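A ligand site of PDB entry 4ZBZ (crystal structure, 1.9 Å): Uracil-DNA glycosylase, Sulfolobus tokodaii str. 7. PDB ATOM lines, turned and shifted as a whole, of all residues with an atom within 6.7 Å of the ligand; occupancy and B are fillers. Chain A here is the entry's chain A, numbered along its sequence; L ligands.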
ATOM      1  N   GLU A  10     -23.774 -27.018 -26.028  1.00  0.00           N
ATOM      2  CA  GLU A  10     -22.879 -25.867 -25.983  1.00  0.00           C
ATOM      3  C   GLU A  10     -21.465 -26.313 -26.343  1.00  0.00           C
ATOM      4  O   GLU A  10     -20.767 -25.668 -27.125  1.00  0.00           O
ATOM      5  CB  GLU A  10     -22.898 -25.213 -24.604  1.00  0.00           C
ATOM      6  CG  GLU A  10     -24.182 -24.472 -24.298  1.00  0.00           C
ATOM      7  CD  GLU A  10     -24.185 -23.812 -22.934  1.00  0.00           C
ATOM      8  OE1 GLU A  10     -23.113 -23.475 -22.400  1.00  0.00           O
ATOM      9  OE2 GLU A  10     -25.292 -23.615 -22.380  1.00  0.00           O
ATOM     10  N   VAL A  11     -21.042 -27.409 -25.733  1.00  0.00           N
ATOM     11  CA  VAL A  11     -19.694 -27.913 -25.962  1.00  0.00           C
ATOM     12  C   VAL A  11     -19.442 -28.243 -27.435  1.00  0.00           C
ATOM     13  O   VAL A  11     -18.378 -27.889 -27.980  1.00  0.00           O
ATOM     14  CB  VAL A  11     -19.426 -29.177 -25.133  1.00  0.00           C
ATOM     15  CG1 VAL A  11     -18.148 -29.887 -25.625  1.00  0.00           C
ATOM     16  CG2 VAL A  11     -19.312 -28.794 -23.674  1.00  0.00           C
ATOM     17  N   ILE A  12     -20.382 -28.903 -28.105  1.00  0.00           N
ATOM     18  CA  ILE A  12     -20.015 -29.404 -29.430  1.00  0.00           C
ATOM     19  C   ILE A  12     -19.893 -28.290 -30.458  1.00  0.00           C
ATOM     20  O   ILE A  12     -19.177 -28.459 -31.456  1.00  0.00           O
ATOM     21  CB  ILE A  12     -20.988 -30.484 -29.928  1.00  0.00           C
ATOM     22  CG1 ILE A  12     -22.407 -29.939 -30.040  1.00  0.00           C
ATOM     23  CG2 ILE A  12     -20.886 -31.725 -29.029  1.00  0.00           C
ATOM     24  CD1 ILE A  12     -23.414 -30.968 -30.531  1.00  0.00           C
ATOM     25  N   SER A  13     -20.503 -27.133 -30.194  1.00  0.00           N
ATOM     26  CA  SER A  13     -20.310 -26.004 -31.084  1.00  0.00           C
ATOM     27  C   SER A  13     -19.530 -24.893 -30.407  1.00  0.00           C
ATOM     28  O   SER A  13     -19.520 -23.762 -30.879  1.00  0.00           O
ATOM     29  CB  SER A  13     -21.649 -25.480 -31.583  1.00  0.00           C
ATOM     30  OG  SER A  13     -22.433 -25.038 -30.489  1.00  0.00           O
ATOM     31  N   CYS A  14     -18.848 -25.232 -29.310  1.00  0.00           N
ATOM     32  CA  CYS A  14     -18.148 -24.216 -28.521  1.00  0.00           C
ATOM     33  C   CYS A  14     -16.910 -23.635 -29.208  1.00  0.00           C
ATOM     34  O   CYS A  14     -16.090 -24.378 -29.731  1.00  0.00           O
ATOM     35  CB  CYS A  14     -17.729 -24.818 -27.174  1.00  0.00           C
ATOM     36  SG  CYS A  14     -16.984 -23.605 -26.066  1.00  0.00           S
ATOM     37  N   LYS A  15     -16.780 -22.303 -29.183  1.00  0.00           N
ATOM     38  CA  LYS A  15     -15.563 -21.656 -29.681  1.00  0.00           C
ATOM     39  C   LYS A  15     -14.997 -20.671 -28.651  1.00  0.00           C
ATOM     40  O   LYS A  15     -14.487 -19.610 -28.998  1.00  0.00           O
ATOM     41  CB  LYS A  15     -15.853 -20.974 -31.002  1.00  0.00           C
ATOM     42  CG  LYS A  15     -16.318 -21.942 -32.086  1.00  0.00           C
ATOM     43  CD  LYS A  15     -16.494 -21.312 -33.454  1.00  0.00           C
ATOM     44  CE  LYS A  15     -17.016 -22.356 -34.447  1.00  0.00           C
ATOM     45  NZ  LYS A  15     -17.442 -21.778 -35.747  1.00  0.00           N
ATOM     46  N   LYS A  16     -15.106 -21.034 -27.364  1.00  0.00           N
ATOM     47  CA  LYS A  16     -14.767 -20.135 -26.262  1.00  0.00           C
ATOM     48  C   LYS A  16     -13.282 -20.079 -25.915  1.00  0.00           C
ATOM     49  O   LYS A  16     -12.869 -19.182 -25.169  1.00  0.00           O
ATOM     50  CB  LYS A  16     -15.542 -20.546 -25.003  1.00  0.00           C
ATOM     51  CG  LYS A  16     -17.014 -20.194 -25.006  1.00  0.00           C
ATOM     52  CD  LYS A  16     -17.667 -20.656 -23.718  1.00  0.00           C
ATOM     53  CE  LYS A  16     -19.184 -20.502 -23.767  1.00  0.00           C
ATOM     54  NZ  LYS A  16     -19.849 -21.287 -22.688  1.00  0.00           N
ATOM     55  N   CYS A  17     -12.475 -21.010 -26.421  1.00  0.00           N
ATOM     56  CA  CYS A  17     -11.015 -20.833 -26.339  1.00  0.00           C
ATOM     57  C   CYS A  17     -10.366 -21.271 -27.639  1.00  0.00           C
ATOM     58  O   CYS A  17     -11.041 -21.764 -28.559  1.00  0.00           O
ATOM     59  CB  CYS A  17     -10.421 -21.592 -25.139  1.00  0.00           C
ATOM     60  SG  CYS A  17     -10.087 -23.356 -25.365  1.00  0.00           S
ATOM     61  N   LYS A  18      -9.052 -21.105 -27.747  1.00  0.00           N
ATOM     62  CA  LYS A  18      -8.414 -21.311 -29.043  1.00  0.00           C
ATOM     63  C   LYS A  18      -8.333 -22.784 -29.444  1.00  0.00           C
ATOM     64  O   LYS A  18      -7.954 -23.091 -30.585  1.00  0.00           O
ATOM     65  CB  LYS A  18      -7.001 -20.692 -29.049  1.00  0.00           C
ATOM     66  CG  LYS A  18      -6.070 -21.226 -27.977  1.00  0.00           C
ATOM     67  CD  LYS A  18      -4.734 -20.475 -28.000  1.00  0.00           C
ATOM     68  CE  LYS A  18      -3.797 -20.953 -26.909  1.00  0.00           C
ATOM     69  NZ  LYS A  18      -4.452 -20.924 -25.564  1.00  0.00           N
ATOM     70  N   LEU A  19      -8.683 -23.695 -28.530  1.00  0.00           N
ATOM     71  CA  LEU A  19      -8.591 -25.122 -28.849  1.00  0.00           C
ATOM     72  C   LEU A  19      -9.602 -25.537 -29.919  1.00  0.00           C
ATOM     73  O   LEU A  19      -9.384 -26.518 -30.651  1.00  0.00           O
ATOM     74  CB  LEU A  19      -8.769 -25.992 -27.589  1.00  0.00           C
ATOM     75  CG  LEU A  19      -7.645 -25.875 -26.553  1.00  0.00           C
ATOM     76  CD1 LEU A  19      -7.799 -26.896 -25.398  1.00  0.00           C
ATOM     77  CD2 LEU A  19      -6.292 -26.010 -27.250  1.00  0.00           C
ATOM     78  N   TRP A  20     -10.686 -24.781 -30.035  1.00  0.00           N
ATOM     79  CA  TRP A  20     -11.748 -25.153 -30.968  1.00  0.00           C
ATOM     80  C   TRP A  20     -11.216 -25.345 -32.398  1.00  0.00           C
ATOM     81  O   TRP A  20     -11.664 -26.235 -33.111  1.00  0.00           O
ATOM     82  CB  TRP A  20     -12.863 -24.099 -30.954  1.00  0.00           C
ATOM     83  CG  TRP A  20     -12.569 -22.911 -31.809  1.00  0.00           C
ATOM     84  CD1 TRP A  20     -11.935 -21.766 -31.442  1.00  0.00           C
ATOM     85  CD2 TRP A  20     -12.898 -22.756 -33.193  1.00  0.00           C
ATOM     86  NE1 TRP A  20     -11.840 -20.897 -32.516  1.00  0.00           N
ATOM     87  CE2 TRP A  20     -12.419 -21.491 -33.609  1.00  0.00           C
ATOM     88  CE3 TRP A  20     -13.550 -23.560 -34.132  1.00  0.00           C
ATOM     89  CZ2 TRP A  20     -12.583 -21.017 -34.909  1.00  0.00           C
ATOM     90  CZ3 TRP A  20     -13.701 -23.092 -35.429  1.00  0.00           C
ATOM     91  CH2 TRP A  20     -13.226 -21.830 -35.795  1.00  0.00           C
ATOM     92  N   GLN A  21     -10.238 -24.533 -32.798  1.00  0.00           N
ATOM     93  CA  GLN A  21      -9.770 -24.536 -34.182  1.00  0.00           C
ATOM     94  C   GLN A  21      -9.070 -25.829 -34.562  1.00  0.00           C
ATOM     95  O   GLN A  21      -8.869 -26.095 -35.750  1.00  0.00           O
ATOM     96  CB  GLN A  21      -8.798 -23.365 -34.427  1.00  0.00           C
ATOM     97  CG  GLN A  21      -7.512 -23.495 -33.604  1.00  0.00           C
ATOM     98  CD  GLN A  21      -6.612 -22.277 -33.718  1.00  0.00           C
ATOM     99  OE1 GLN A  21      -6.029 -22.026 -34.756  1.00  0.00           O
ATOM    100  NE2 GLN A  21      -6.503 -21.530 -32.626  1.00  0.00           N
ATOM    101  N   ARG A  23      -9.889 -29.077 -33.533  1.00  0.00           N
ATOM    102  CA  ARG A  23     -10.602 -30.333 -33.266  1.00  0.00           C
ATOM    103  C   ARG A  23     -11.324 -30.895 -34.469  1.00  0.00           C
ATOM    104  O   ARG A  23     -11.636 -30.170 -35.436  1.00  0.00           O
ATOM    105  CB  ARG A  23     -11.612 -30.137 -32.119  1.00  0.00           C
ATOM    106  CG  ARG A  23     -12.870 -29.369 -32.566  1.00  0.00           C
ATOM    107  CD  ARG A  23     -13.817 -29.063 -31.398  1.00  0.00           C
ATOM    108  NE  ARG A  23     -14.900 -28.186 -31.856  1.00  0.00           N
ATOM    109  CZ  ARG A  23     -15.353 -27.134 -31.172  1.00  0.00           C
ATOM    110  NH1 ARG A  23     -14.819 -26.825 -29.989  1.00  0.00           N
ATOM    111  NH2 ARG A  23     -16.325 -26.385 -31.686  1.00  0.00           N
ATOM    112  N   ALA A  26     -15.515 -31.863 -30.452  1.00  0.00           N
ATOM    113  CA  ALA A  26     -15.389 -31.604 -29.026  1.00  0.00           C
ATOM    114  C   ALA A  26     -15.830 -32.857 -28.294  1.00  0.00           C
ATOM    115  O   ALA A  26     -16.538 -33.696 -28.855  1.00  0.00           O
ATOM    116  CB  ALA A  26     -16.232 -30.419 -28.594  1.00  0.00           C
ATOM    117  N   VAL A  27     -15.446 -32.969 -27.025  1.00  0.00           N
ATOM    118  CA  VAL A  27     -15.757 -34.173 -26.271  1.00  0.00           C
ATOM    119  C   VAL A  27     -16.508 -33.816 -25.010  1.00  0.00           C
ATOM    120  O   VAL A  27     -15.890 -33.560 -23.987  1.00  0.00           O
ATOM    121  CB  VAL A  27     -14.479 -34.954 -25.903  1.00  0.00           C
ATOM    122  CG1 VAL A  27     -14.846 -36.265 -25.230  1.00  0.00           C
ATOM    123  CG2 VAL A  27     -13.613 -35.204 -27.161  1.00  0.00           C
ATOM    124  N   VAL A  83     -11.499 -32.371 -17.906  1.00  0.00           N
ATOM    125  CA  VAL A  83     -11.524 -31.005 -17.418  1.00  0.00           C
ATOM    126  C   VAL A  83     -11.510 -30.027 -18.608  1.00  0.00           C
ATOM    127  O   VAL A  83     -12.167 -28.993 -18.570  1.00  0.00           O
ATOM    128  CB  VAL A  83     -10.347 -30.762 -16.415  1.00  0.00           C
ATOM    129  CG1 VAL A  83      -9.007 -31.083 -17.064  1.00  0.00           C
ATOM    130  CG2 VAL A  83     -10.398 -29.354 -15.826  1.00  0.00           C
ATOM    131  N   VAL A  84     -10.806 -30.393 -19.685  1.00  0.00           N
ATOM    132  CA  VAL A  84     -10.799 -29.631 -20.912  1.00  0.00           C
ATOM    133  C   VAL A  84     -11.376 -30.534 -21.999  1.00  0.00           C
ATOM    134  O   VAL A  84     -11.005 -31.698 -22.071  1.00  0.00           O
ATOM    135  CB  VAL A  84      -9.378 -29.155 -21.288  1.00  0.00           C
ATOM    136  CG1 VAL A  84      -9.364 -28.613 -22.696  1.00  0.00           C
ATOM    137  CG2 VAL A  84      -8.896 -28.094 -20.294  1.00  0.00           C
ATOM    138  N   LYS A  85     -12.253 -30.014 -22.848  1.00  0.00           N
ATOM    139  CA  LYS A  85     -13.040 -30.913 -23.711  1.00  0.00           C
ATOM    140  C   LYS A  85     -12.686 -30.905 -25.200  1.00  0.00           C
ATOM    141  O   LYS A  85     -13.360 -31.580 -26.016  1.00  0.00           O
ATOM    142  CB  LYS A  85     -14.519 -30.608 -23.502  1.00  0.00           C
ATOM    143  CG  LYS A  85     -14.955 -30.957 -22.055  1.00  0.00           C
ATOM    144  CD  LYS A  85     -16.266 -30.344 -21.657  1.00  0.00           C
ATOM    145  CE  LYS A  85     -16.951 -31.169 -20.536  1.00  0.00           C
ATOM    146  NZ  LYS A  85     -16.203 -31.240 -19.232  1.00  0.00           N
ATOM    147  N   CYS A  86     -11.591 -30.210 -25.549  1.00  0.00           N
ATOM    148  CA  CYS A  86     -11.050 -30.260 -26.897  1.00  0.00           C
ATOM    149  C   CYS A  86      -9.563 -30.639 -26.841  1.00  0.00           C
ATOM    150  O   CYS A  86      -8.860 -30.264 -25.906  1.00  0.00           O
ATOM    151  CB  CYS A  86     -11.220 -28.918 -27.605  1.00  0.00           C
ATOM    152  SG  CYS A  86     -12.943 -28.582 -28.016  1.00  0.00           S
ATOM    153  N   ARG A  87      -9.094 -31.362 -27.849  1.00  0.00           N
ATOM    154  CA  ARG A  87      -7.714 -31.834 -27.835  1.00  0.00           C
ATOM    155  C   ARG A  87      -6.736 -30.682 -28.080  1.00  0.00           C
ATOM    156  O   ARG A  87      -6.847 -29.998 -29.099  1.00  0.00           O
ATOM    157  CB  ARG A  87      -7.508 -32.912 -28.896  1.00  0.00           C
ATOM    158  CG  ARG A  87      -6.075 -33.450 -28.937  1.00  0.00           C
ATOM    159  CD  ARG A  87      -5.937 -34.543 -29.977  1.00  0.00           C
ATOM    160  NE  ARG A  87      -6.045 -33.994 -31.326  1.00  0.00           N
ATOM    161  CZ  ARG A  87      -5.002 -33.541 -32.021  1.00  0.00           C
ATOM    162  NH1 ARG A  87      -3.778 -33.596 -31.500  1.00  0.00           N
ATOM    163  NH2 ARG A  87      -5.182 -33.063 -33.241  1.00  0.00           N
ATOM    164  N   GLU A  98      -7.172 -22.026 -21.039  1.00  0.00           N
ATOM    165  CA  GLU A  98      -8.033 -23.051 -21.635  1.00  0.00           C
ATOM    166  C   GLU A  98      -8.772 -23.790 -20.519  1.00  0.00           C
ATOM    167  O   GLU A  98      -9.983 -24.033 -20.601  1.00  0.00           O
ATOM    168  CB  GLU A  98      -7.201 -24.001 -22.502  1.00  0.00           C
ATOM    169  CG  GLU A  98      -6.563 -23.279 -23.701  1.00  0.00           C
ATOM    170  CD  GLU A  98      -5.419 -24.038 -24.342  1.00  0.00           C
ATOM    171  OE1 GLU A  98      -4.974 -25.072 -23.802  1.00  0.00           O
ATOM    172  OE2 GLU A  98      -4.956 -23.586 -25.413  1.00  0.00           O
ATOM    173  N   ALA A 101     -11.300 -21.388 -19.411  1.00  0.00           N
ATOM    174  CA  ALA A 101     -12.409 -21.264 -20.362  1.00  0.00           C
ATOM    175  C   ALA A 101     -13.371 -22.441 -20.272  1.00  0.00           C
ATOM    176  O   ALA A 101     -14.585 -22.268 -20.348  1.00  0.00           O
ATOM    177  CB  ALA A 101     -11.867 -21.132 -21.783  1.00  0.00           C
ATOM    178  N   CYS A 102     -12.830 -23.638 -20.111  1.00  0.00           N
ATOM    179  CA  CYS A 102     -13.600 -24.858 -20.286  1.00  0.00           C
ATOM    180  C   CYS A 102     -14.152 -25.399 -18.978  1.00  0.00           C
ATOM    181  O   CYS A 102     -15.235 -26.012 -18.962  1.00  0.00           O
ATOM    182  CB  CYS A 102     -12.753 -25.933 -20.954  1.00  0.00           C
ATOM    183  SG  CYS A 102     -13.754 -27.277 -21.680  1.00  0.00           S
ATOM    184  N   SER A 103     -13.420 -25.207 -17.889  1.00  0.00           N
ATOM    185  CA  SER A 103     -13.805 -25.845 -16.640  1.00  0.00           C
ATOM    186  C   SER A 103     -15.233 -25.534 -16.153  1.00  0.00           C
ATOM    187  O   SER A 103     -15.793 -26.361 -15.447  1.00  0.00           O
ATOM    188  CB  SER A 103     -12.807 -25.499 -15.519  1.00  0.00           C
ATOM    189  OG  SER A 103     -12.718 -24.110 -15.300  1.00  0.00           O
ATOM    190  N   TYR A 105     -17.828 -25.881 -17.719  1.00  0.00           N
ATOM    191  CA  TYR A 105     -18.649 -26.989 -18.209  1.00  0.00           C
ATOM    192  C   TYR A 105     -18.610 -28.138 -17.223  1.00  0.00           C
ATOM    193  O   TYR A 105     -19.643 -28.745 -16.888  1.00  0.00           O
ATOM    194  CB  TYR A 105     -18.178 -27.472 -19.564  1.00  0.00           C
ATOM    195  CG  TYR A 105     -18.475 -26.526 -20.721  1.00  0.00           C
ATOM    196  CD1 TYR A 105     -17.476 -26.194 -21.622  1.00  0.00           C
ATOM    197  CD2 TYR A 105     -19.748 -26.001 -20.919  1.00  0.00           C
ATOM    198  CE1 TYR A 105     -17.738 -25.364 -22.688  1.00  0.00           C
ATOM    199  CE2 TYR A 105     -20.023 -25.165 -22.019  1.00  0.00           C
ATOM    200  CZ  TYR A 105     -19.004 -24.847 -22.895  1.00  0.00           C
ATOM    201  OH  TYR A 105     -19.223 -24.032 -23.971  1.00  0.00           O
HETATM  202 FE1  LIG L   1     -12.238 -24.511 -25.392  1.00  0.00          FE
HETATM  203 FE2  LIG L   1     -14.898 -24.713 -25.673  1.00  0.00          FE
HETATM  204 FE3  LIG L   1     -13.279 -26.755 -26.496  1.00  0.00          FE
HETATM  205 FE4  LIG L   1     -13.663 -26.261 -23.858  1.00  0.00          FE
HETATM  206  S1  LIG L   1     -15.255 -26.946 -25.303  1.00  0.00           S
HETATM  207  S2  LIG L   1     -11.676 -26.709 -24.902  1.00  0.00           S
HETATM  208  S3  LIG L   1     -13.815 -23.956 -23.852  1.00  0.00           S
HETATM  209  S4  LIG L   1     -13.349 -24.625 -27.355  1.00  0.00           S
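Merely in contact with the ligand: Lys 16 (3.99 Å), Leu 19 (3.9 Å), Val 84 (3.7 Å), Lys 85 (3.9 Å), Ala 101 (3.9 Å) and Tyr 105 (3.9 Å).
12 residues have an atom within 4 Å of the ligand: Cys 14, Lys 16, Cys 17, Leu 19, Trp 20, Arg 23, Val 84, Lys 85, Cys 86, Ala 101, Cys 102 and Tyr 105.
N of Trp 20 sits close to S4 of the ligand (3.8 Å).
NH1 of Arg 23 sits close to S4 of the ligand (3.7 Å).
S2 of the ligand lies close to N of Cys 86.
An iron atom (FE4) of the ligand is bound by the side-chain sulfur (SG) of Cys 102 (2.4 Å).
An iron atom (FE1) of the ligand is bound by the side-chain sulfur (SG) of Cys 17 (2.4 Å).
An iron atom (FE3) of the ligand is bound by the side-chain sulfur (SG) of Cys 86 (2.4 Å).
FE2 of the ligand is bound by SG of Cys 14 (2.4 Å).
SG of Cys 86 sits close to NH1 of Arg 23, 3.2 Å away.
The backbone NH of Lys 85 sits close to the side-chain sulfur of Cys 102, 3.3 Å away.
NH1 of Arg 23 is in hydrogen-bond range of O of Cys 14 (2.8 Å).
The side-chain hydroxyl (OH) of Tyr 105 lies close to the side-chain sulfur (SG) of Cys 14 (3.1 Å).
The backbone NH of Leu 19 lies close to the side-chain sulfur of Cys 17 (3.5 Å).
The side-chain carboxylate (OE1) of Glu 10 lies within salt-bridge range of the side-chain amino group (NZ) of Lys 16, 3.9 Å away.
OH of Tyr 105 sits at hydrogen-bond distance from NZ of Lys 16.
SG of Cys 14 lies close to N of Lys 16 (3.4 Å).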
